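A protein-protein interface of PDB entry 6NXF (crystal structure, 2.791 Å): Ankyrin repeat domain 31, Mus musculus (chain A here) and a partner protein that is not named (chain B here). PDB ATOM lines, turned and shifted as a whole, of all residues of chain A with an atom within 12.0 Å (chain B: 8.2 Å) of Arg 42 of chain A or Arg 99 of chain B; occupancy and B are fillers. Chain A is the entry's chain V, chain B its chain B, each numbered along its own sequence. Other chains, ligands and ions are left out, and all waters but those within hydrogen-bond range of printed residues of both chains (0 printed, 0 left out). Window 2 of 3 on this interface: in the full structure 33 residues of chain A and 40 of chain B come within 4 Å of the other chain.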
ATOM      1  N   GLN A  34       0.984 -29.055  -4.827  1.00  0.00           N
ATOM      2  CA  GLN A  34       0.636 -27.712  -5.255  1.00  0.00           C
ATOM      3  C   GLN A  34       1.026 -26.718  -4.164  1.00  0.00           C
ATOM      4  O   GLN A  34       1.892 -25.853  -4.365  1.00  0.00           O
ATOM      5  CB  GLN A  34      -0.858 -27.645  -5.583  1.00  0.00           C
ATOM      6  N   HIS A  35       0.449 -26.889  -2.963  1.00  0.00           N
ATOM      7  CA  HIS A  35       0.690 -25.952  -1.877  1.00  0.00           C
ATOM      8  C   HIS A  35       2.169 -25.884  -1.525  1.00  0.00           C
ATOM      9  O   HIS A  35       2.669 -24.819  -1.169  1.00  0.00           O
ATOM     10  CB  HIS A  35      -0.142 -26.340  -0.653  1.00  0.00           C
ATOM     11  CG  HIS A  35      -1.625 -26.118  -0.804  1.00  0.00           C
ATOM     12  ND1 HIS A  35      -2.526 -27.155  -0.964  1.00  0.00           N
ATOM     13  CD2 HIS A  35      -2.368 -24.982  -0.786  1.00  0.00           C
ATOM     14  CE1 HIS A  35      -3.754 -26.670  -1.053  1.00  0.00           C
ATOM     15  NE2 HIS A  35      -3.687 -25.354  -0.947  1.00  0.00           N
ATOM     16  N   TRP A  36       2.892 -26.996  -1.646  1.00  0.00           N
ATOM     17  CA  TRP A  36       4.341 -26.992  -1.422  1.00  0.00           C
ATOM     18  C   TRP A  36       5.055 -26.059  -2.393  1.00  0.00           C
ATOM     19  O   TRP A  36       5.848 -25.202  -1.981  1.00  0.00           O
ATOM     20  CB  TRP A  36       4.895 -28.418  -1.556  1.00  0.00           C
ATOM     21  CG  TRP A  36       6.407 -28.542  -1.395  1.00  0.00           C
ATOM     22  CD1 TRP A  36       7.336 -28.595  -2.386  1.00  0.00           C
ATOM     23  CD2 TRP A  36       7.129 -28.634  -0.165  1.00  0.00           C
ATOM     24  NE1 TRP A  36       8.597 -28.707  -1.852  1.00  0.00           N
ATOM     25  CE2 TRP A  36       8.497 -28.733  -0.489  1.00  0.00           C
ATOM     26  CE3 TRP A  36       6.751 -28.635   1.176  1.00  0.00           C
ATOM     27  CZ2 TRP A  36       9.488 -28.837   0.479  1.00  0.00           C
ATOM     28  CZ3 TRP A  36       7.728 -28.738   2.131  1.00  0.00           C
ATOM     29  CH2 TRP A  36       9.085 -28.841   1.785  1.00  0.00           C
ATOM     30  N   LYS A  37       4.758 -26.203  -3.692  1.00  0.00           N
ATOM     31  CA  LYS A  37       5.487 -25.483  -4.728  1.00  0.00           C
ATOM     32  C   LYS A  37       5.364 -23.980  -4.543  1.00  0.00           C
ATOM     33  O   LYS A  37       6.342 -23.248  -4.747  1.00  0.00           O
ATOM     34  CB  LYS A  37       4.981 -25.904  -6.104  1.00  0.00           C
ATOM     35  N   PHE A  38       4.172 -23.504  -4.148  1.00  0.00           N
ATOM     36  CA  PHE A  38       3.961 -22.105  -3.775  1.00  0.00           C
ATOM     37  C   PHE A  38       5.079 -21.593  -2.853  1.00  0.00           C
ATOM     38  O   PHE A  38       5.814 -20.656  -3.196  1.00  0.00           O
ATOM     39  CB  PHE A  38       2.572 -21.975  -3.118  1.00  0.00           C
ATOM     40  CG  PHE A  38       2.146 -20.544  -2.770  1.00  0.00           C
ATOM     41  CD1 PHE A  38       2.783 -19.811  -1.764  1.00  0.00           C
ATOM     42  CD2 PHE A  38       1.059 -19.961  -3.407  1.00  0.00           C
ATOM     43  CE1 PHE A  38       2.375 -18.515  -1.446  1.00  0.00           C
ATOM     44  CE2 PHE A  38       0.648 -18.674  -3.085  1.00  0.00           C
ATOM     45  CZ  PHE A  38       1.310 -17.953  -2.103  1.00  0.00           C
ATOM     46  N   TYR A  39       5.234 -22.202  -1.677  1.00  0.00           N
ATOM     47  CA  TYR A  39       6.265 -21.701  -0.781  1.00  0.00           C
ATOM     48  C   TYR A  39       7.660 -21.913  -1.351  1.00  0.00           C
ATOM     49  O   TYR A  39       8.584 -21.193  -0.961  1.00  0.00           O
ATOM     50  CB  TYR A  39       6.119 -22.341   0.604  1.00  0.00           C
ATOM     51  CG  TYR A  39       4.745 -22.096   1.183  1.00  0.00           C
ATOM     52  CD1 TYR A  39       3.692 -22.945   0.879  1.00  0.00           C
ATOM     53  CD2 TYR A  39       4.484 -20.985   1.996  1.00  0.00           C
ATOM     54  CE1 TYR A  39       2.418 -22.714   1.380  1.00  0.00           C
ATOM     55  CE2 TYR A  39       3.210 -20.745   2.513  1.00  0.00           C
ATOM     56  CZ  TYR A  39       2.177 -21.613   2.198  1.00  0.00           C
ATOM     57  OH  TYR A  39       0.892 -21.395   2.681  1.00  0.00           O
ATOM     58  N   VAL A  40       7.832 -22.841  -2.297  1.00  0.00           N
ATOM     59  CA  VAL A  40       9.165 -23.075  -2.852  1.00  0.00           C
ATOM     60  C   VAL A  40       9.657 -21.854  -3.618  1.00  0.00           C
ATOM     61  O   VAL A  40      10.733 -21.317  -3.331  1.00  0.00           O
ATOM     62  CB  VAL A  40       9.182 -24.315  -3.764  1.00  0.00           C
ATOM     63  CG1 VAL A  40      10.584 -24.463  -4.379  1.00  0.00           C
ATOM     64  CG2 VAL A  40       8.757 -25.571  -3.009  1.00  0.00           C
ATOM     65  N   GLY A  41       8.867 -21.399  -4.598  1.00  0.00           N
ATOM     66  CA  GLY A  41       9.383 -20.544  -5.654  1.00  0.00           C
ATOM     67  C   GLY A  41       9.870 -19.199  -5.150  1.00  0.00           C
ATOM     68  O   GLY A  41       9.572 -18.767  -4.033  1.00  0.00           O
ATOM     69  N   ARG A  42      10.655 -18.524  -6.005  1.00  0.00           N
ATOM     70  CA  ARG A  42      11.175 -17.211  -5.626  1.00  0.00           C
ATOM     71  C   ARG A  42      10.062 -16.162  -5.572  1.00  0.00           C
ATOM     72  O   ARG A  42      10.152 -15.210  -4.785  1.00  0.00           O
ATOM     73  CB  ARG A  42      12.305 -16.781  -6.579  1.00  0.00           C
ATOM     74  CG  ARG A  42      11.952 -15.708  -7.636  1.00  0.00           C
ATOM     75  CD  ARG A  42      12.253 -14.269  -7.148  1.00  0.00           C
ATOM     76  NE  ARG A  42      12.134 -13.234  -8.188  1.00  0.00           N
ATOM     77  CZ  ARG A  42      11.095 -12.414  -8.337  1.00  0.00           C
ATOM     78  NH1 ARG A  42      10.050 -12.497  -7.520  1.00  0.00           N
ATOM     79  NH2 ARG A  42      11.098 -11.509  -9.306  1.00  0.00           N
ATOM     80  N   SER A  43       8.999 -16.327  -6.373  1.00  0.00           N
ATOM     81  CA  SER A  43       7.903 -15.362  -6.347  1.00  0.00           C
ATOM     82  C   SER A  43       7.355 -15.199  -4.939  1.00  0.00           C
ATOM     83  O   SER A  43       6.954 -14.100  -4.537  1.00  0.00           O
ATOM     84  CB  SER A  43       6.781 -15.785  -7.304  1.00  0.00           C
ATOM     85  OG  SER A  43       6.183 -17.014  -6.911  1.00  0.00           O
ATOM     86  N   HIS A  44       7.361 -16.277  -4.157  1.00  0.00           N
ATOM     87  CA  HIS A  44       6.802 -16.242  -2.814  1.00  0.00           C
ATOM     88  C   HIS A  44       7.875 -16.375  -1.735  1.00  0.00           C
ATOM     89  O   HIS A  44       7.568 -16.737  -0.593  1.00  0.00           O
ATOM     90  CB  HIS A  44       5.727 -17.319  -2.697  1.00  0.00           C
ATOM     91  CG  HIS A  44       4.759 -17.299  -3.837  1.00  0.00           C
ATOM     92  ND1 HIS A  44       4.341 -16.125  -4.432  1.00  0.00           N
ATOM     93  CD2 HIS A  44       4.159 -18.302  -4.522  1.00  0.00           C
ATOM     94  CE1 HIS A  44       3.510 -16.406  -5.421  1.00  0.00           C
ATOM     95  NE2 HIS A  44       3.378 -17.719  -5.493  1.00  0.00           N
ATOM     96  N   SER A  45       9.133 -16.091  -2.073  1.00  0.00           N
ATOM     97  CA  SER A  45      10.118 -15.812  -1.036  1.00  0.00           C
ATOM     98  C   SER A  45       9.621 -14.632  -0.212  1.00  0.00           C
ATOM     99  O   SER A  45       9.157 -13.630  -0.767  1.00  0.00           O
ATOM    100  CB  SER A  45      11.500 -15.523  -1.644  1.00  0.00           C
ATOM    101  OG  SER A  45      11.448 -14.581  -2.713  1.00  0.00           O
ATOM    102  N   GLU A  46       9.687 -14.776   1.113  1.00  0.00           N
ATOM    103  CA  GLU A  46       9.115 -13.919   2.149  1.00  0.00           C
ATOM    104  C   GLU A  46       7.644 -14.278   2.455  1.00  0.00           C
ATOM    105  O   GLU A  46       7.141 -13.868   3.503  1.00  0.00           O
ATOM    106  CB  GLU A  46       9.225 -12.409   1.837  1.00  0.00           C
ATOM    107  N   ALA A  47       6.947 -15.037   1.591  1.00  0.00           N
ATOM    108  CA  ALA A  47       5.604 -15.548   1.876  1.00  0.00           C
ATOM    109  C   ALA A  47       5.608 -16.689   2.891  1.00  0.00           C
ATOM    110  O   ALA A  47       4.536 -17.086   3.373  1.00  0.00           O
ATOM    111  CB  ALA A  47       4.927 -16.033   0.589  1.00  0.00           C
ATOM    112  N   LEU A  48       6.784 -17.237   3.203  1.00  0.00           N
ATOM    113  CA  LEU A  48       6.945 -18.219   4.258  1.00  0.00           C
ATOM    114  C   LEU A  48       7.166 -17.570   5.613  1.00  0.00           C
ATOM    115  O   LEU A  48       6.953 -18.230   6.637  1.00  0.00           O
ATOM    116  CB  LEU A  48       8.124 -19.139   3.926  1.00  0.00           C
ATOM    117  CG  LEU A  48       8.160 -20.585   4.434  1.00  0.00           C
ATOM    118  CD1 LEU A  48       8.679 -20.666   5.843  1.00  0.00           C
ATOM    119  CD2 LEU A  48       6.789 -21.223   4.345  1.00  0.00           C
ATOM    120  N   LEU A  49       7.592 -16.303   5.650  1.00  0.00           N
ATOM    121  CA  LEU A  49       7.731 -15.573   6.905  1.00  0.00           C
ATOM    122  C   LEU A  49       6.475 -14.784   7.241  1.00  0.00           C
ATOM    123  O   LEU A  49       6.532 -13.841   8.041  1.00  0.00           O
ATOM    124  CB  LEU A  49       8.950 -14.648   6.862  1.00  0.00           C
ATOM    125  CG  LEU A  49       9.560 -14.250   8.211  1.00  0.00           C
ATOM    126  CD1 LEU A  49      11.057 -14.514   8.205  1.00  0.00           C
ATOM    127  CD2 LEU A  49       9.273 -12.785   8.588  1.00  0.00           C
ATOM    128  N   SER A  50       5.339 -15.167   6.657  1.00  0.00           N
ATOM    129  CA  SER A  50       4.085 -14.449   6.856  1.00  0.00           C
ATOM    130  C   SER A  50       3.673 -14.426   8.329  1.00  0.00           C
ATOM    131  O   SER A  50       3.797 -13.386   8.990  1.00  0.00           O
ATOM    132  CB  SER A  50       2.976 -15.049   5.975  1.00  0.00           C
ATOM    133  OG  SER A  50       2.850 -16.455   6.140  1.00  0.00           O
ATOM    134  N   TRP A  51       3.191 -15.553   8.858  1.00  0.00           N
ATOM    135  CA  TRP A  51       2.675 -15.633  10.241  1.00  0.00           C
ATOM    136  C   TRP A  51       1.523 -14.647  10.480  1.00  0.00           C
ATOM    137  O   TRP A  51       0.957 -14.583  11.579  1.00  0.00           O
ATOM    138  CB  TRP A  51       3.800 -15.393  11.268  1.00  0.00           C
ATOM    139  CG  TRP A  51       4.918 -16.380  11.141  1.00  0.00           C
ATOM    140  CD1 TRP A  51       6.187 -16.139  10.692  1.00  0.00           C
ATOM    141  CD2 TRP A  51       4.858 -17.775  11.440  1.00  0.00           C
ATOM    142  NE1 TRP A  51       6.924 -17.299  10.698  1.00  0.00           N
ATOM    143  CE2 TRP A  51       6.131 -18.320  11.157  1.00  0.00           C
ATOM    144  CE3 TRP A  51       3.854 -18.618  11.933  1.00  0.00           C
ATOM    145  CZ2 TRP A  51       6.425 -19.670  11.344  1.00  0.00           C
ATOM    146  CZ3 TRP A  51       4.141 -19.952  12.112  1.00  0.00           C
ATOM    147  CH2 TRP A  51       5.423 -20.468  11.828  1.00  0.00           C
ATOM    148  N   ILE B  96      12.419 -31.124   3.408  1.00  0.00           N
ATOM    149  CA  ILE B  96      12.371 -29.845   4.095  1.00  0.00           C
ATOM    150  C   ILE B  96      13.124 -28.813   3.261  1.00  0.00           C
ATOM    151  O   ILE B  96      14.094 -29.146   2.569  1.00  0.00           O
ATOM    152  CB  ILE B  96      12.931 -29.954   5.531  1.00  0.00           C
ATOM    153  CG1 ILE B  96      14.401 -29.601   5.593  1.00  0.00           C
ATOM    154  CG2 ILE B  96      12.758 -31.382   6.084  1.00  0.00           C
ATOM    155  CD1 ILE B  96      15.083 -30.316   6.722  1.00  0.00           C
ATOM    156  N   VAL B  97      12.650 -27.563   3.301  1.00  0.00           N
ATOM    157  CA  VAL B  97      13.186 -26.472   2.489  1.00  0.00           C
ATOM    158  C   VAL B  97      13.335 -25.229   3.356  1.00  0.00           C
ATOM    159  O   VAL B  97      12.403 -24.848   4.071  1.00  0.00           O
ATOM    160  CB  VAL B  97      12.295 -26.166   1.262  1.00  0.00           C
ATOM    161  CG1 VAL B  97      10.828 -25.922   1.666  1.00  0.00           C
ATOM    162  CG2 VAL B  97      12.867 -24.983   0.454  1.00  0.00           C
ATOM    163  N   ARG B  98      14.488 -24.589   3.272  1.00  0.00           N
ATOM    164  CA  ARG B  98      14.803 -23.427   4.084  1.00  0.00           C
ATOM    165  C   ARG B  98      14.449 -22.146   3.336  1.00  0.00           C
ATOM    166  O   ARG B  98      14.519 -22.083   2.104  1.00  0.00           O
ATOM    167  CB  ARG B  98      16.290 -23.449   4.444  1.00  0.00           C
ATOM    168  CG  ARG B  98      16.678 -22.628   5.646  1.00  0.00           C
ATOM    169  CD  ARG B  98      16.948 -21.200   5.305  1.00  0.00           C
ATOM    170  NE  ARG B  98      18.276 -20.774   5.723  1.00  0.00           N
ATOM    171  CZ  ARG B  98      19.218 -20.376   4.875  1.00  0.00           C
ATOM    172  NH1 ARG B  98      18.959 -20.351   3.571  1.00  0.00           N
ATOM    173  NH2 ARG B  98      20.404 -19.990   5.323  1.00  0.00           N
ATOM    174  N   ARG B  99      14.037 -21.132   4.093  1.00  0.00           N
ATOM    175  CA  ARG B  99      13.922 -19.766   3.582  1.00  0.00           C
ATOM    176  C   ARG B  99      14.255 -18.822   4.722  1.00  0.00           C
ATOM    177  O   ARG B  99      13.531 -18.777   5.721  1.00  0.00           O
ATOM    178  CB  ARG B  99      12.530 -19.456   3.026  1.00  0.00           C
ATOM    179  CG  ARG B  99      12.365 -19.765   1.545  1.00  0.00           C
ATOM    180  CD  ARG B  99      12.694 -18.566   0.659  1.00  0.00           C
ATOM    181  NE  ARG B  99      12.022 -18.664  -0.637  1.00  0.00           N
ATOM    182  CZ  ARG B  99      12.558 -19.218  -1.721  1.00  0.00           C
ATOM    183  NH1 ARG B  99      13.789 -19.722  -1.674  1.00  0.00           N
ATOM    184  NH2 ARG B  99      11.862 -19.264  -2.853  1.00  0.00           N
ATOM    185  N   MET B 100      15.348 -18.085   4.569  1.00  0.00           N
ATOM    186  CA  MET B 100      15.847 -17.204   5.611  1.00  0.00           C
ATOM    187  C   MET B 100      16.041 -17.932   6.944  1.00  0.00           C
ATOM    188  O   MET B 100      16.884 -18.823   7.085  1.00  0.00           O
ATOM    189  CB  MET B 100      14.893 -16.023   5.807  1.00  0.00           C
ATOM    190  CG  MET B 100      14.615 -15.233   4.541  1.00  0.00           C
ATOM    191  SD  MET B 100      16.189 -14.281   3.930  1.00  0.00           S
ATOM    192  CE  MET B 100      16.814 -13.630   5.663  1.00  0.00           C
ATOM    193  N   ASP B 101      15.256 -17.509   7.928  1.00  0.00           N
ATOM    194  CA  ASP B 101      15.274 -18.079   9.263  1.00  0.00           C
ATOM    195  C   ASP B 101      14.029 -18.922   9.512  1.00  0.00           C
ATOM    196  O   ASP B 101      13.489 -18.942  10.619  1.00  0.00           O
ATOM    197  CB  ASP B 101      15.409 -16.967  10.298  1.00  0.00           C
ATOM    198  CG  ASP B 101      14.392 -15.861  10.093  1.00  0.00           C
ATOM    199  OD1 ASP B 101      13.575 -15.981   9.157  1.00  0.00           O
ATOM    200  OD2 ASP B 101      14.399 -14.877  10.860  1.00  0.00           O
ATOM    201  N   CYS B 102      13.555 -19.606   8.482  1.00  0.00           N
ATOM    202  CA  CYS B 102      12.394 -20.470   8.596  1.00  0.00           C
ATOM    203  C   CYS B 102      12.634 -21.771   7.845  1.00  0.00           C
ATOM    204  O   CYS B 102      13.188 -21.780   6.741  1.00  0.00           O
ATOM    205  CB  CYS B 102      11.157 -19.782   8.060  1.00  0.00           C
ATOM    206  SG  CYS B 102      10.788 -18.214   8.865  1.00  0.00           S
ATOM    207  N   LEU B 103      12.229 -22.870   8.462  1.00  0.00           N
ATOM    208  CA  LEU B 103      12.220 -24.168   7.820  1.00  0.00           C
ATOM    209  C   LEU B 103      10.785 -24.581   7.548  1.00  0.00           C
ATOM    210  O   LEU B 103       9.915 -24.451   8.411  1.00  0.00           O
ATOM    211  CB  LEU B 103      12.907 -25.199   8.703  1.00  0.00           C
ATOM    212  CG  LEU B 103      14.413 -25.009   8.773  1.00  0.00           C
ATOM    213  CD1 LEU B 103      15.026 -25.974   9.778  1.00  0.00           C
ATOM    214  CD2 LEU B 103      14.979 -25.220   7.373  1.00  0.00           C
ATOM    215  N   LEU B 104      10.525 -25.052   6.346  1.00  0.00           N
ATOM    216  CA  LEU B 104       9.247 -25.655   6.014  1.00  0.00           C
ATOM    217  C   LEU B 104       9.454 -27.155   5.848  1.00  0.00           C
ATOM    218  O   LEU B 104      10.396 -27.582   5.174  1.00  0.00           O
ATOM    219  CB  LEU B 104       8.681 -25.037   4.742  1.00  0.00           C
ATOM    220  CG  LEU B 104       7.533 -25.800   4.099  1.00  0.00           C
ATOM    221  CD1 LEU B 104       6.314 -25.822   5.010  1.00  0.00           C
ATOM    222  CD2 LEU B 104       7.194 -25.175   2.755  1.00  0.00           C
ATOM    223  N   VAL B 118       8.425 -23.469  10.918  1.00  0.00           N
ATOM    224  CA  VAL B 118       9.040 -23.064  12.167  1.00  0.00           C
ATOM    225  C   VAL B 118       9.877 -21.811  11.910  1.00  0.00           C
ATOM    226  O   VAL B 118      10.455 -21.648  10.831  1.00  0.00           O
ATOM    227  CB  VAL B 118       9.865 -24.241  12.733  1.00  0.00           C
ATOM    228  CG1 VAL B 118      11.060 -24.573  11.811  1.00  0.00           C
ATOM    229  CG2 VAL B 118      10.334 -23.913  14.067  1.00  0.00           C
ATOM    230  N   GLN B 119       9.913 -20.908  12.893  1.00  0.00           N
ATOM    231  CA  GLN B 119      10.746 -19.708  12.830  1.00  0.00           C
ATOM    232  C   GLN B 119      11.626 -19.670  14.066  1.00  0.00           C
ATOM    233  O   GLN B 119      11.117 -19.666  15.194  1.00  0.00           O
ATOM    234  CB  GLN B 119       9.908 -18.432  12.735  1.00  0.00           C
ATOM    235  CG  GLN B 119      10.747 -17.159  12.683  1.00  0.00           C
ATOM    236  CD  GLN B 119       9.927 -15.918  12.333  1.00  0.00           C
ATOM    237  OE1 GLN B 119       8.837 -15.702  12.876  1.00  0.00           O
ATOM    238  NE2 GLN B 119      10.449 -15.100  11.414  1.00  0.00           N
ATOM    239  N   PHE B 120      12.941 -19.638  13.849  1.00  0.00           N
ATOM    240  CA  PHE B 120      13.890 -19.815  14.942  1.00  0.00           C
ATOM    241  C   PHE B 120      13.976 -18.565  15.797  1.00  0.00           C
ATOM    242  O   PHE B 120      14.029 -17.446  15.286  1.00  0.00           O
ATOM    243  CB  PHE B 120      15.266 -20.157  14.399  1.00  0.00           C
ATOM    244  CG  PHE B 120      15.369 -21.551  13.917  1.00  0.00           C
ATOM    245  CD1 PHE B 120      15.863 -22.552  14.750  1.00  0.00           C
ATOM    246  CD2 PHE B 120      14.957 -21.875  12.628  1.00  0.00           C
ATOM    247  CE1 PHE B 120      15.962 -23.857  14.300  1.00  0.00           C
ATOM    248  CE2 PHE B 120      15.055 -23.169  12.157  1.00  0.00           C
ATOM    249  CZ  PHE B 120      15.555 -24.172  12.996  1.00  0.00           C
ATOM    250  N   LEU B 129      18.948 -15.911  12.523  1.00  0.00           N
ATOM    251  CA  LEU B 129      19.357 -16.525  11.264  1.00  0.00           C
ATOM    252  C   LEU B 129      20.457 -17.551  11.497  1.00  0.00           C
ATOM    253  O   LEU B 129      20.459 -18.624  10.879  1.00  0.00           O
ATOM    254  CB  LEU B 129      19.817 -15.447  10.284  1.00  0.00           C
ATOM    255  CG  LEU B 129      19.904 -15.844   8.815  1.00  0.00           C
ATOM    256  CD1 LEU B 129      21.253 -16.460   8.471  1.00  0.00           C
ATOM    257  CD2 LEU B 129      18.776 -16.800   8.471  1.00  0.00           C
ATOM    258  N   CYS B 132      19.015 -20.899  12.911  1.00  0.00           N
ATOM    259  CA  CYS B 132      18.407 -21.650  11.816  1.00  0.00           C
ATOM    260  C   CYS B 132      19.476 -22.308  10.967  1.00  0.00           C
ATOM    261  O   CYS B 132      19.373 -23.486  10.612  1.00  0.00           O
ATOM    262  CB  CYS B 132      17.538 -20.763  10.928  1.00  0.00           C
ATOM    263  SG  CYS B 132      16.860 -21.709   9.490  1.00  0.00           S
ATOM    264  N   VAL B 145      18.770 -30.443   2.497  1.00  0.00           N
ATOM    265  CA  VAL B 145      17.882 -29.349   2.857  1.00  0.00           C
ATOM    266  C   VAL B 145      17.941 -28.341   1.722  1.00  0.00           C
ATOM    267  O   VAL B 145      18.935 -27.621   1.592  1.00  0.00           O
ATOM    268  CB  VAL B 145      18.283 -28.703   4.185  1.00  0.00           C
ATOM    269  CG1 VAL B 145      17.350 -27.538   4.509  1.00  0.00           C
ATOM    270  CG2 VAL B 145      18.334 -29.742   5.302  1.00  0.00           C
ATOM    271  N   GLN B 146      16.887 -28.284   0.902  1.00  0.00           N
ATOM    272  CA  GLN B 146      16.793 -27.267  -0.146  1.00  0.00           C
ATOM    273  C   GLN B 146      17.097 -25.901   0.458  1.00  0.00           C
ATOM    274  O   GLN B 146      16.702 -25.594   1.586  1.00  0.00           O
ATOM    275  CB  GLN B 146      15.397 -27.287  -0.800  1.00  0.00           C
ATOM    276  CG  GLN B 146      15.195 -26.361  -2.027  1.00  0.00           C
ATOM    277  CD  GLN B 146      13.820 -26.544  -2.747  1.00  0.00           C
ATOM    278  OE1 GLN B 146      13.002 -27.397  -2.370  1.00  0.00           O
ATOM    279  NE2 GLN B 146      13.582 -25.736  -3.787  1.00  0.00           N
ATOM    280  N   GLU B 147      17.880 -25.098  -0.276  1.00  0.00           N
ATOM    281  CA  GLU B 147      18.406 -23.836   0.233  1.00  0.00           C
ATOM    282  C   GLU B 147      18.659 -22.955  -0.987  1.00  0.00           C
ATOM    283  O   GLU B 147      19.686 -23.106  -1.668  1.00  0.00           O
ATOM    284  CB  GLU B 147      19.670 -24.059   1.062  1.00  0.00           C
ATOM    285  CG  GLU B 147      19.944 -22.987   2.102  1.00  0.00           C
ATOM    286  CD  GLU B 147      21.008 -23.404   3.112  1.00  0.00           C
ATOM    287  OE1 GLU B 147      21.744 -24.373   2.836  1.00  0.00           O
ATOM    288  OE2 GLU B 147      21.102 -22.775   4.191  1.00  0.00           O
ATOM    289  N   PRO B 148      17.749 -22.009  -1.281  1.00  0.00           N
ATOM    290  CA  PRO B 148      17.388 -21.340  -2.544  1.00  0.00           C
ATOM    291  C   PRO B 148      18.330 -21.573  -3.743  1.00  0.00           C
ATOM    292  O   PRO B 148      19.419 -20.992  -3.836  1.00  0.00           O
ATOM    293  CB  PRO B 148      17.369 -19.866  -2.142  1.00  0.00           C
ATOM    294  CG  PRO B 148      16.967 -19.895  -0.650  1.00  0.00           C
ATOM    295  CD  PRO B 148      17.150 -21.311  -0.131  1.00  0.00           C
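O of Gly 41 of chain A lies within hydrogen-bond range of NH2 of Arg 99 of chain B, 2.6 Å away. The side-chain amide oxygen of Gln 119 of chain B is in hydrogen-bond range of the indole nitrogen of Trp 51 of chain A (3.3 Å). The backbone carbonyl oxygen (O) of Val 40 of chain A sits close to the guanidinium group (NH2) of Arg 99 of chain B, 2.4 Å away. The backbone NH (N) of Arg 42 of chain A sits close to the guanidinium group (NH2) of Arg 99 of chain B, 3.5 Å away.
N of Gln 146 of chain B sits at hydrogen-bond distance from O of Ile 96 of chain B, 3.4 Å away. The backbone NH of Val 97 of chain B sits at hydrogen-bond distance from the backbone carbonyl oxygen of Leu 104 of chain B, 2.9 Å away. The backbone NH (N) of Arg 98 of chain B lies within hydrogen-bond range of the backbone carbonyl oxygen (O) of Gln 146 of chain B (3.0 Å). OD1 of Asp 101 of chain B lies close to SG of Cys 102 of chain B (3.6 Å). The backbone carbonyl oxygen (O) of Asp 101 of chain B sits at hydrogen-bond distance from the backbone NH (N) of Phe 120 of chain B. O of Arg 42 of chain A sits at hydrogen-bond distance from OG of Ser 45 of chain A (2.5 Å).
CG1 of Val 97 of chain B touches CH2 of Trp 36 of chain A (3.4 Å). Leu 104 of chain B touches Trp 36 of chain A (CG to CZ3, 3.5 Å). Leu 104 of chain B touches Tyr 39 of chain A. Val 40 of chain A touches Gln 146 of chain B (CG1 to NE2, 3.3 Å). Ser 45 of chain A touches Arg 99 of chain B (CB to NE, 3.3 Å). Leu 48 of chain A touches Cys 102 of chain B. Asp 101 of chain B touches Leu 49 of chain A. CD1 of Leu 49 of chain A touches SG of Cys 102 of chain B, 3.8 Å away. CD1 of Leu 49 of chain A touches NE2 of Gln 119 of chain B, 3.3 Å away.
Printed residues of chain B within 4 Å of Trp 36 of chain A: Val 97 and Leu 104. Of the printed residues of chain B, Tyr 39 of chain A touches Leu 104. Gly 41 of chain A touches just one residue of chain B: Arg 99. Printed residues of chain B within 4 Å of Ser 45 of chain A: Arg 99 (3.3 Å). Of the printed residues of chain B, Leu 48 of chain A touches Cys 102. Val 97 of chain B touches one residue of chain A. No residue of chain A comes within 4 Å of Arg 98 of chain B. Arg 99 of chain B touches just these residues of chain A: Val 40, Gly 41, Arg 42 and Ser 45. Cys 102 of chain B touches just these residues of chain A: Leu 48 (3.4 Å) and Leu 49 (3.8 Å). No residue of chain A comes within 4 Å of Leu 103 of chain B. The nearest residue of chain B that does not touch Arg 42 of chain A is Pro 148 of chain B (7.4 Å). The nearest printed residue of chain A that does not touch Gln 119 of chain B is Leu 48 of chain A (6.7 Å).
Of the 18 printed residues of chain A, 9 touch a printed residue of chain B. Among the printed residues, 13 pairs touch across the chains.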
